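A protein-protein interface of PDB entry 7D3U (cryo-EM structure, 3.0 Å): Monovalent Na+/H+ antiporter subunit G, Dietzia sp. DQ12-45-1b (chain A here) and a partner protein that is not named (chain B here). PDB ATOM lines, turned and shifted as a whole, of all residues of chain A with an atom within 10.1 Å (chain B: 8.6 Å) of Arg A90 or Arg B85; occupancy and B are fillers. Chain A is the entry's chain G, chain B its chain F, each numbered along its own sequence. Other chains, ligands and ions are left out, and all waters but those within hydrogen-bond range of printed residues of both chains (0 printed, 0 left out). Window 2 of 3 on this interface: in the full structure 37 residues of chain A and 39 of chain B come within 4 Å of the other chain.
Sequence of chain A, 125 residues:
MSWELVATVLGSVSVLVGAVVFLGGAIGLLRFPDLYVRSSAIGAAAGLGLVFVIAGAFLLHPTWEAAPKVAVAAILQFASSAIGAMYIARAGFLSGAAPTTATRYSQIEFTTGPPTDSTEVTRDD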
ATOM      1  N   LEU A  35      22.338   4.586  27.266  1.00  0.00           N
ATOM      2  CA  LEU A  35      21.135   3.921  26.785  1.00  0.00           C
ATOM      3  C   LEU A  35      21.480   2.703  25.947  1.00  0.00           C
ATOM      4  O   LEU A  35      20.722   1.728  25.929  1.00  0.00           O
ATOM      5  CB  LEU A  35      20.285   4.895  25.965  1.00  0.00           C
ATOM      6  CG  LEU A  35      18.945   4.424  25.392  1.00  0.00           C
ATOM      7  CD1 LEU A  35      18.003   5.593  25.314  1.00  0.00           C
ATOM      8  CD2 LEU A  35      19.099   3.810  24.013  1.00  0.00           C
ATOM      9  N   TYR A  36      22.615   2.745  25.250  1.00  0.00           N
ATOM     10  CA  TYR A  36      22.996   1.654  24.364  1.00  0.00           C
ATOM     11  C   TYR A  36      23.561   0.478  25.145  1.00  0.00           C
ATOM     12  O   TYR A  36      23.357  -0.677  24.760  1.00  0.00           O
ATOM     13  CB  TYR A  36      23.996   2.162  23.329  1.00  0.00           C
ATOM     14  CG  TYR A  36      23.574   3.479  22.726  1.00  0.00           C
ATOM     15  CD1 TYR A  36      22.602   3.530  21.740  1.00  0.00           C
ATOM     16  CD2 TYR A  36      24.131   4.671  23.159  1.00  0.00           C
ATOM     17  CE1 TYR A  36      22.207   4.728  21.194  1.00  0.00           C
ATOM     18  CE2 TYR A  36      23.742   5.873  22.619  1.00  0.00           C
ATOM     19  CZ  TYR A  36      22.779   5.897  21.638  1.00  0.00           C
ATOM     20  OH  TYR A  36      22.388   7.096  21.096  1.00  0.00           O
ATOM     21  N   SER A  39      20.376  -1.077  26.510  1.00  0.00           N
ATOM     22  CA  SER A  39      19.664  -1.859  25.506  1.00  0.00           C
ATOM     23  C   SER A  39      20.429  -3.125  25.147  1.00  0.00           C
ATOM     24  O   SER A  39      19.822  -4.175  24.909  1.00  0.00           O
ATOM     25  CB  SER A  39      19.413  -1.012  24.262  1.00  0.00           C
ATOM     26  OG  SER A  39      18.688   0.160  24.586  1.00  0.00           O
ATOM     27  N   SER A  40      21.760  -3.050  25.107  1.00  0.00           N
ATOM     28  CA  SER A  40      22.558  -4.233  24.810  1.00  0.00           C
ATOM     29  C   SER A  40      22.422  -5.283  25.901  1.00  0.00           C
ATOM     30  O   SER A  40      22.463  -6.484  25.613  1.00  0.00           O
ATOM     31  CB  SER A  40      24.025  -3.845  24.630  1.00  0.00           C
ATOM     32  OG  SER A  40      24.583  -3.394  25.849  1.00  0.00           O
ATOM     33  N   ALA A  82      14.990  -9.278  20.867  1.00  0.00           N
ATOM     34  CA  ALA A  82      16.066  -8.729  20.050  1.00  0.00           C
ATOM     35  C   ALA A  82      15.612  -7.468  19.321  1.00  0.00           C
ATOM     36  O   ALA A  82      16.251  -6.411  19.419  1.00  0.00           O
ATOM     37  CB  ALA A  82      16.561  -9.777  19.059  1.00  0.00           C
ATOM     38  N   ILE A  83      14.491  -7.558  18.601  1.00  0.00           N
ATOM     39  CA  ILE A  83      14.091  -6.484  17.697  1.00  0.00           C
ATOM     40  C   ILE A  83      13.624  -5.258  18.472  1.00  0.00           C
ATOM     41  O   ILE A  83      13.898  -4.120  18.074  1.00  0.00           O
ATOM     42  CB  ILE A  83      13.015  -6.995  16.726  1.00  0.00           C
ATOM     43  CG1 ILE A  83      13.636  -7.992  15.755  1.00  0.00           C
ATOM     44  CG2 ILE A  83      12.382  -5.847  15.962  1.00  0.00           C
ATOM     45  CD1 ILE A  83      12.652  -8.609  14.819  1.00  0.00           C
ATOM     46  N   GLY A  84      12.902  -5.461  19.576  1.00  0.00           N
ATOM     47  CA  GLY A  84      12.466  -4.329  20.373  1.00  0.00           C
ATOM     48  C   GLY A  84      13.630  -3.517  20.900  1.00  0.00           C
ATOM     49  O   GLY A  84      13.636  -2.289  20.813  1.00  0.00           O
ATOM     50  N   ALA A  85      14.642  -4.197  21.442  1.00  0.00           N
ATOM     51  CA  ALA A  85      15.820  -3.491  21.932  1.00  0.00           C
ATOM     52  C   ALA A  85      16.574  -2.821  20.792  1.00  0.00           C
ATOM     53  O   ALA A  85      17.065  -1.696  20.943  1.00  0.00           O
ATOM     54  CB  ALA A  85      16.734  -4.454  22.687  1.00  0.00           C
ATOM     55  N   MET A  86      16.665  -3.491  19.639  1.00  0.00           N
ATOM     56  CA  MET A  86      17.324  -2.890  18.484  1.00  0.00           C
ATOM     57  C   MET A  86      16.660  -1.575  18.099  1.00  0.00           C
ATOM     58  O   MET A  86      17.329  -0.546  17.936  1.00  0.00           O
ATOM     59  CB  MET A  86      17.300  -3.865  17.307  1.00  0.00           C
ATOM     60  CG  MET A  86      18.413  -4.887  17.334  1.00  0.00           C
ATOM     61  SD  MET A  86      17.939  -6.469  16.621  1.00  0.00           S
ATOM     62  CE  MET A  86      17.118  -5.923  15.133  1.00  0.00           C
ATOM     63  N   TYR A  87      15.333  -1.585  17.972  1.00  0.00           N
ATOM     64  CA  TYR A  87      14.634  -0.384  17.537  1.00  0.00           C
ATOM     65  C   TYR A  87      14.610   0.682  18.621  1.00  0.00           C
ATOM     66  O   TYR A  87      14.637   1.875  18.305  1.00  0.00           O
ATOM     67  CB  TYR A  87      13.215  -0.728  17.093  1.00  0.00           C
ATOM     68  CG  TYR A  87      13.143  -1.179  15.657  1.00  0.00           C
ATOM     69  CD1 TYR A  87      14.200  -0.955  14.788  1.00  0.00           C
ATOM     70  CD2 TYR A  87      12.022  -1.829  15.169  1.00  0.00           C
ATOM     71  CE1 TYR A  87      14.140  -1.365  13.478  1.00  0.00           C
ATOM     72  CE2 TYR A  87      11.954  -2.242  13.860  1.00  0.00           C
ATOM     73  CZ  TYR A  87      13.016  -2.009  13.018  1.00  0.00           C
ATOM     74  OH  TYR A  87      12.950  -2.421  11.711  1.00  0.00           O
ATOM     75  N   ILE A  88      14.575   0.286  19.894  1.00  0.00           N
ATOM     76  CA  ILE A  88      14.651   1.274  20.966  1.00  0.00           C
ATOM     77  C   ILE A  88      15.997   1.984  20.933  1.00  0.00           C
ATOM     78  O   ILE A  88      16.067   3.212  21.047  1.00  0.00           O
ATOM     79  CB  ILE A  88      14.390   0.614  22.332  1.00  0.00           C
ATOM     80  CG1 ILE A  88      12.913   0.250  22.473  1.00  0.00           C
ATOM     81  CG2 ILE A  88      14.808   1.537  23.455  1.00  0.00           C
ATOM     82  CD1 ILE A  88      11.990   1.431  22.376  1.00  0.00           C
ATOM     83  N   ALA A  89      17.083   1.229  20.756  1.00  0.00           N
ATOM     84  CA  ALA A  89      18.400   1.852  20.675  1.00  0.00           C
ATOM     85  C   ALA A  89      18.510   2.757  19.455  1.00  0.00           C
ATOM     86  O   ALA A  89      19.059   3.863  19.540  1.00  0.00           O
ATOM     87  CB  ALA A  89      19.488   0.781  20.648  1.00  0.00           C
ATOM     88  N   ARG A  90      17.989   2.309  18.310  1.00  0.00           N
ATOM     89  CA  ARG A  90      18.060   3.131  17.105  1.00  0.00           C
ATOM     90  C   ARG A  90      17.277   4.427  17.279  1.00  0.00           C
ATOM     91  O   ARG A  90      17.770   5.511  16.943  1.00  0.00           O
ATOM     92  CB  ARG A  90      17.542   2.349  15.901  1.00  0.00           C
ATOM     93  CG  ARG A  90      17.464   3.177  14.636  1.00  0.00           C
ATOM     94  CD  ARG A  90      16.164   2.934  13.905  1.00  0.00           C
ATOM     95  NE  ARG A  90      15.997   3.844  12.779  1.00  0.00           N
ATOM     96  CZ  ARG A  90      14.884   3.948  12.064  1.00  0.00           C
ATOM     97  NH1 ARG A  90      13.833   3.197  12.360  1.00  0.00           N
ATOM     98  NH2 ARG A  90      14.819   4.803  11.053  1.00  0.00           N
ATOM     99  N   ALA A  91      16.053   4.336  17.802  1.00  0.00           N
ATOM    100  CA  ALA A  91      15.248   5.533  18.013  1.00  0.00           C
ATOM    101  C   ALA A  91      15.861   6.446  19.065  1.00  0.00           C
ATOM    102  O   ALA A  91      15.710   7.669  18.983  1.00  0.00           O
ATOM    103  CB  ALA A  91      13.825   5.146  18.409  1.00  0.00           C
ATOM    104  N   GLY A  92      16.551   5.879  20.056  1.00  0.00           N
ATOM    105  CA  GLY A  92      17.254   6.714  21.013  1.00  0.00           C
ATOM    106  C   GLY A  92      18.402   7.464  20.372  1.00  0.00           C
ATOM    107  O   GLY A  92      18.629   8.640  20.664  1.00  0.00           O
ATOM    108  N   PHE A  93      19.134   6.797  19.477  1.00  0.00           N
ATOM    109  CA  PHE A  93      20.169   7.488  18.717  1.00  0.00           C
ATOM    110  C   PHE A  93      19.568   8.614  17.888  1.00  0.00           C
ATOM    111  O   PHE A  93      20.095   9.733  17.861  1.00  0.00           O
ATOM    112  CB  PHE A  93      20.914   6.502  17.820  1.00  0.00           C
ATOM    113  CG  PHE A  93      21.954   7.146  16.947  1.00  0.00           C
ATOM    114  CD1 PHE A  93      21.614   7.694  15.722  1.00  0.00           C
ATOM    115  CD2 PHE A  93      23.274   7.201  17.353  1.00  0.00           C
ATOM    116  CE1 PHE A  93      22.566   8.281  14.922  1.00  0.00           C
ATOM    117  CE2 PHE A  93      24.229   7.789  16.555  1.00  0.00           C
ATOM    118  CZ  PHE A  93      23.873   8.332  15.340  1.00  0.00           C
ATOM    119  N   LEU A  94      18.465   8.332  17.195  1.00  0.00           N
ATOM    120  CA  LEU A  94      17.834   9.353  16.366  1.00  0.00           C
ATOM    121  C   LEU A  94      17.288  10.496  17.211  1.00  0.00           C
ATOM    122  O   LEU A  94      17.445  11.668  16.853  1.00  0.00           O
ATOM    123  CB  LEU A  94      16.726   8.732  15.521  1.00  0.00           C
ATOM    124  CG  LEU A  94      17.198   7.867  14.356  1.00  0.00           C
ATOM    125  CD1 LEU A  94      16.039   7.533  13.437  1.00  0.00           C
ATOM    126  CD2 LEU A  94      18.300   8.573  13.593  1.00  0.00           C
ATOM    127  N   SER A  95      16.647  10.179  18.337  1.00  0.00           N
ATOM    128  CA  SER A  95      16.085  11.225  19.182  1.00  0.00           C
ATOM    129  C   SER A  95      17.159  12.033  19.899  1.00  0.00           C
ATOM    130  O   SER A  95      16.856  13.109  20.425  1.00  0.00           O
ATOM    131  CB  SER A  95      15.126  10.619  20.204  1.00  0.00           C
ATOM    132  OG  SER A  95      14.607  11.618  21.063  1.00  0.00           O
ATOM    133  N   GLY A  96      18.394  11.545  19.936  1.00  0.00           N
ATOM    134  CA  GLY A  96      19.478  12.296  20.537  1.00  0.00           C
ATOM    135  C   GLY A  96      19.924  11.786  21.891  1.00  0.00           C
ATOM    136  O   GLY A  96      20.252  12.582  22.776  1.00  0.00           O
ATOM    137  N   ALA A  97      19.943  10.468  22.073  1.00  0.00           N
ATOM    138  CA  ALA A  97      20.435   9.888  23.318  1.00  0.00           C
ATOM    139  C   ALA A  97      21.948  10.038  23.371  1.00  0.00           C
ATOM    140  O   ALA A  97      22.671   9.404  22.597  1.00  0.00           O
ATOM    141  CB  ALA A  97      20.031   8.422  23.426  1.00  0.00           C
ATOM    142  N   ILE A 108      30.342   6.369  14.227  1.00  0.00           N
ATOM    143  CA  ILE A 108      29.047   6.908  13.835  1.00  0.00           C
ATOM    144  C   ILE A 108      28.922   8.290  14.455  1.00  0.00           C
ATOM    145  O   ILE A 108      29.011   8.435  15.679  1.00  0.00           O
ATOM    146  CB  ILE A 108      27.887   6.009  14.289  1.00  0.00           C
ATOM    147  CG1 ILE A 108      27.960   4.658  13.585  1.00  0.00           C
ATOM    148  CG2 ILE A 108      26.563   6.668  13.989  1.00  0.00           C
ATOM    149  CD1 ILE A 108      27.779   4.760  12.101  1.00  0.00           C
ATOM    150  N   GLU A 109      28.716   9.302  13.618  1.00  0.00           N
ATOM    151  CA  GLU A 109      28.634  10.665  14.117  1.00  0.00           C
ATOM    152  C   GLU A 109      27.299  10.907  14.808  1.00  0.00           C
ATOM    153  O   GLU A 109      26.276  10.313  14.461  1.00  0.00           O
ATOM    154  CB  GLU A 109      28.826  11.664  12.978  1.00  0.00           C
ATOM    155  CG  GLU A 109      30.180  11.574  12.295  1.00  0.00           C
ATOM    156  CD  GLU A 109      31.327  11.978  13.204  1.00  0.00           C
ATOM    157  OE1 GLU A 109      31.738  11.162  14.056  1.00  0.00           O
ATOM    158  OE2 GLU A 109      31.820  13.117  13.063  1.00  0.00           O
ATOM    159  N   PHE A 110      27.317  11.795  15.796  1.00  0.00           N
ATOM    160  CA  PHE A 110      26.141  12.096  16.603  1.00  0.00           C
ATOM    161  C   PHE A 110      25.580  13.487  16.363  1.00  0.00           C
ATOM    162  O   PHE A 110      24.359  13.652  16.344  1.00  0.00           O
ATOM    163  CB  PHE A 110      26.472  11.938  18.091  1.00  0.00           C
ATOM    164  CG  PHE A 110      26.566  10.511  18.540  1.00  0.00           C
ATOM    165  CD1 PHE A 110      27.744   9.800  18.390  1.00  0.00           C
ATOM    166  CD2 PHE A 110      25.476   9.878  19.111  1.00  0.00           C
ATOM    167  CE1 PHE A 110      27.832   8.485  18.803  1.00  0.00           C
ATOM    168  CE2 PHE A 110      25.560   8.565  19.526  1.00  0.00           C
ATOM    169  CZ  PHE A 110      26.739   7.867  19.370  1.00  0.00           C
ATOM    170  N   HIS B  27      16.929  10.119  29.831  1.00  0.00           N
ATOM    171  CA  HIS B  27      16.447  10.255  28.467  1.00  0.00           C
ATOM    172  C   HIS B  27      15.171   9.446  28.286  1.00  0.00           C
ATOM    173  O   HIS B  27      14.984   8.400  28.912  1.00  0.00           O
ATOM    174  CB  HIS B  27      17.501   9.794  27.460  1.00  0.00           C
ATOM    175  CG  HIS B  27      17.035   9.845  26.038  1.00  0.00           C
ATOM    176  ND1 HIS B  27      16.548  10.995  25.458  1.00  0.00           N
ATOM    177  CD2 HIS B  27      16.976   8.888  25.084  1.00  0.00           C
ATOM    178  CE1 HIS B  27      16.211  10.746  24.205  1.00  0.00           C
ATOM    179  NE2 HIS B  27      16.461   9.473  23.954  1.00  0.00           N
ATOM    180  N   LEU B  74       7.765  -1.743  19.965  1.00  0.00           N
ATOM    181  CA  LEU B  74       8.075  -1.081  18.702  1.00  0.00           C
ATOM    182  C   LEU B  74       7.405   0.283  18.622  1.00  0.00           C
ATOM    183  O   LEU B  74       8.034   1.279  18.244  1.00  0.00           O
ATOM    184  CB  LEU B  74       7.633  -1.957  17.531  1.00  0.00           C
ATOM    185  CG  LEU B  74       8.221  -3.363  17.454  1.00  0.00           C
ATOM    186  CD1 LEU B  74       7.632  -4.113  16.278  1.00  0.00           C
ATOM    187  CD2 LEU B  74       9.729  -3.306  17.351  1.00  0.00           C
ATOM    188  N   ALA B  77       9.269   2.866  20.369  1.00  0.00           N
ATOM    189  CA  ALA B  77      10.313   3.352  19.477  1.00  0.00           C
ATOM    190  C   ALA B  77       9.745   4.351  18.481  1.00  0.00           C
ATOM    191  O   ALA B  77      10.291   5.445  18.298  1.00  0.00           O
ATOM    192  CB  ALA B  77      10.972   2.179  18.751  1.00  0.00           C
ATOM    193  N   ARG B  78       8.624   3.999  17.849  1.00  0.00           N
ATOM    194  CA  ARG B  78       7.966   4.911  16.921  1.00  0.00           C
ATOM    195  C   ARG B  78       7.586   6.227  17.581  1.00  0.00           C
ATOM    196  O   ARG B  78       7.399   7.228  16.882  1.00  0.00           O
ATOM    197  CB  ARG B  78       6.726   4.242  16.327  1.00  0.00           C
ATOM    198  CG  ARG B  78       6.140   4.960  15.123  1.00  0.00           C
ATOM    199  CD  ARG B  78       7.187   5.182  14.052  1.00  0.00           C
ATOM    200  NE  ARG B  78       7.860   3.943  13.684  1.00  0.00           N
ATOM    201  CZ  ARG B  78       7.429   3.114  12.741  1.00  0.00           C
ATOM    202  NH1 ARG B  78       6.323   3.394  12.069  1.00  0.00           N
ATOM    203  NH2 ARG B  78       8.103   2.007  12.470  1.00  0.00           N
ATOM    204  N   MET B  80       9.584   7.549  20.211  1.00  0.00           N
ATOM    205  CA  MET B  80      10.848   8.226  20.477  1.00  0.00           C
ATOM    206  C   MET B  80      11.384   8.908  19.228  1.00  0.00           C
ATOM    207  O   MET B  80      12.012   9.968  19.321  1.00  0.00           O
ATOM    208  CB  MET B  80      11.873   7.238  21.023  1.00  0.00           C
ATOM    209  CG  MET B  80      11.466   6.607  22.332  1.00  0.00           C
ATOM    210  SD  MET B  80      12.385   5.111  22.708  1.00  0.00           S
ATOM    211  CE  MET B  80      13.995   5.554  22.077  1.00  0.00           C
ATOM    212  N   SER B  81      11.144   8.322  18.059  1.00  0.00           N
ATOM    213  CA  SER B  81      11.534   8.921  16.791  1.00  0.00           C
ATOM    214  C   SER B  81      10.566  10.002  16.334  1.00  0.00           C
ATOM    215  O   SER B  81      10.622  10.408  15.169  1.00  0.00           O
ATOM    216  CB  SER B  81      11.650   7.841  15.716  1.00  0.00           C
ATOM    217  OG  SER B  81      11.706   8.418  14.425  1.00  0.00           O
ATOM    218  N   GLY B  82       9.687  10.467  17.217  1.00  0.00           N
ATOM    219  CA  GLY B  82       8.751  11.518  16.870  1.00  0.00           C
ATOM    220  C   GLY B  82       7.734  11.133  15.823  1.00  0.00           C
ATOM    221  O   GLY B  82       7.186  12.011  15.151  1.00  0.00           O
ATOM    222  N   GLY B  83       7.465   9.842  15.662  1.00  0.00           N
ATOM    223  CA  GLY B  83       6.533   9.391  14.650  1.00  0.00           C
ATOM    224  C   GLY B  83       7.208   9.136  13.322  1.00  0.00           C
ATOM    225  O   GLY B  83       6.746   8.313  12.526  1.00  0.00           O
ATOM    226  N   ARG B  84       8.307   9.842  13.072  1.00  0.00           N
ATOM    227  CA  ARG B  84       9.045   9.669  11.831  1.00  0.00           C
ATOM    228  C   ARG B  84       9.682   8.288  11.783  1.00  0.00           C
ATOM    229  O   ARG B  84      10.274   7.823  12.761  1.00  0.00           O
ATOM    230  CB  ARG B  84      10.120  10.747  11.700  1.00  0.00           C
ATOM    231  CG  ARG B  84       9.574  12.149  11.487  1.00  0.00           C
ATOM    232  CD  ARG B  84      10.678  13.187  11.599  1.00  0.00           C
ATOM    233  NE  ARG B  84      10.266  14.486  11.074  1.00  0.00           N
ATOM    234  CZ  ARG B  84      11.033  15.571  11.083  1.00  0.00           C
ATOM    235  NH1 ARG B  84      12.257  15.516  11.589  1.00  0.00           N
ATOM    236  NH2 ARG B  84      10.579  16.713  10.585  1.00  0.00           N
ATOM    237  N   ARG B  85       9.548   7.627  10.639  1.00  0.00           N
ATOM    238  CA  ARG B  85      10.119   6.302  10.455  1.00  0.00           C
ATOM    239  C   ARG B  85      11.641   6.354  10.494  1.00  0.00           C
ATOM    240  O   ARG B  85      12.253   6.132  11.537  1.00  0.00           O
ATOM    241  CB  ARG B  85       9.650   5.697   9.134  1.00  0.00           C
ATOM    242  CG  ARG B  85       8.357   4.924   9.227  1.00  0.00           C
ATOM    243  CD  ARG B  85       7.167   5.848   9.097  1.00  0.00           C
ATOM    244  NE  ARG B  85       5.909   5.127   9.242  1.00  0.00           N
ATOM    245  CZ  ARG B  85       4.717   5.709   9.263  1.00  0.00           C
ATOM    246  NH1 ARG B  85       4.619   7.025   9.148  1.00  0.00           N
ATOM    247  NH2 ARG B  85       3.625   4.975   9.398  1.00  0.00           N
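O of Arg B85 lies within hydrogen-bond range of NH2 of Arg A90 (2.9 Å).
O of Leu A35 lies within hydrogen-bond range of OG of Ser A39 (2.9 Å).
The side-chain hydroxyl of Tyr A36 lies within hydrogen-bond range of the backbone carbonyl oxygen of Ala A97.
N of Ala A97 is in hydrogen-bond range of O of Gly A92, 2.7 Å away.
CD1 of Leu A35 touches CD2 of His B27, 3.5 Å away.
CD2 of Leu B74 touches CG2 of Ile A83, at 3.9 Å.
CD2 of Tyr A87 touches CD2 of Leu B74, at 3.5 Å.
CD1 of Ile A88 touches N of Ala B77, 3.7 Å away.
O of Ile A88 touches CE of Met B80, at 3.3 Å.
CB of Ala A91 touches O of Ala B77, 3.5 Å away.
N of Gly A92 touches CE of Met B80 (3.3 Å).
Ser A95 touches His B27.
Ser A95 touches Met B80.
His B27 touches Ala A97.
Of chain B, only Arg B85 comes within 4 Å of Arg A90.
Of chain A, only Arg A90 (2.9 Å) comes within 4 Å of Arg B85.
No residue of chain B comes within 4 Å of Ala A89.
Ala A91 touches just these residues of chain B: Ala B77 and Met B80.
Of the printed residues of chain B, Leu A35 touches His B27 (3.5 Å).
Of the printed residues of chain A, Met B80 touches Ile A88 (3.3 Å), Ala A91 (3.7 Å), Gly A92 (3.3 Å) and Ser A95 (3.3 Å).
Of the printed residues of chain A, Ala B77 touches Tyr A87 (3.7 Å), Ile A88 (3.7 Å) and Ala A91 (3.5 Å).
Printed residues of chain B within 4 Å of Ile A88: Ala B77 (3.7 Å) and Met B80 (3.3 Å).
Tyr A36 touches none of the printed residues of chain B.
Ala A85 touches none of the printed residues of chain B.
Of the 10 printed residues of chain B, 5 touch a printed residue of chain A.
Printed residues of chain B that touch a printed residue of chain A: His B27, Leu B74, Ala B77, Met B80 and Arg B85.
Hydrophobic or aromatic side chains of chain A within 4 Å of the printed part of chain B: Leu A35, Ile A83, Tyr A87, Ile A88, Ala A91 and Ala A97.
Among the printed residues, 13 pairs touch across the chains.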
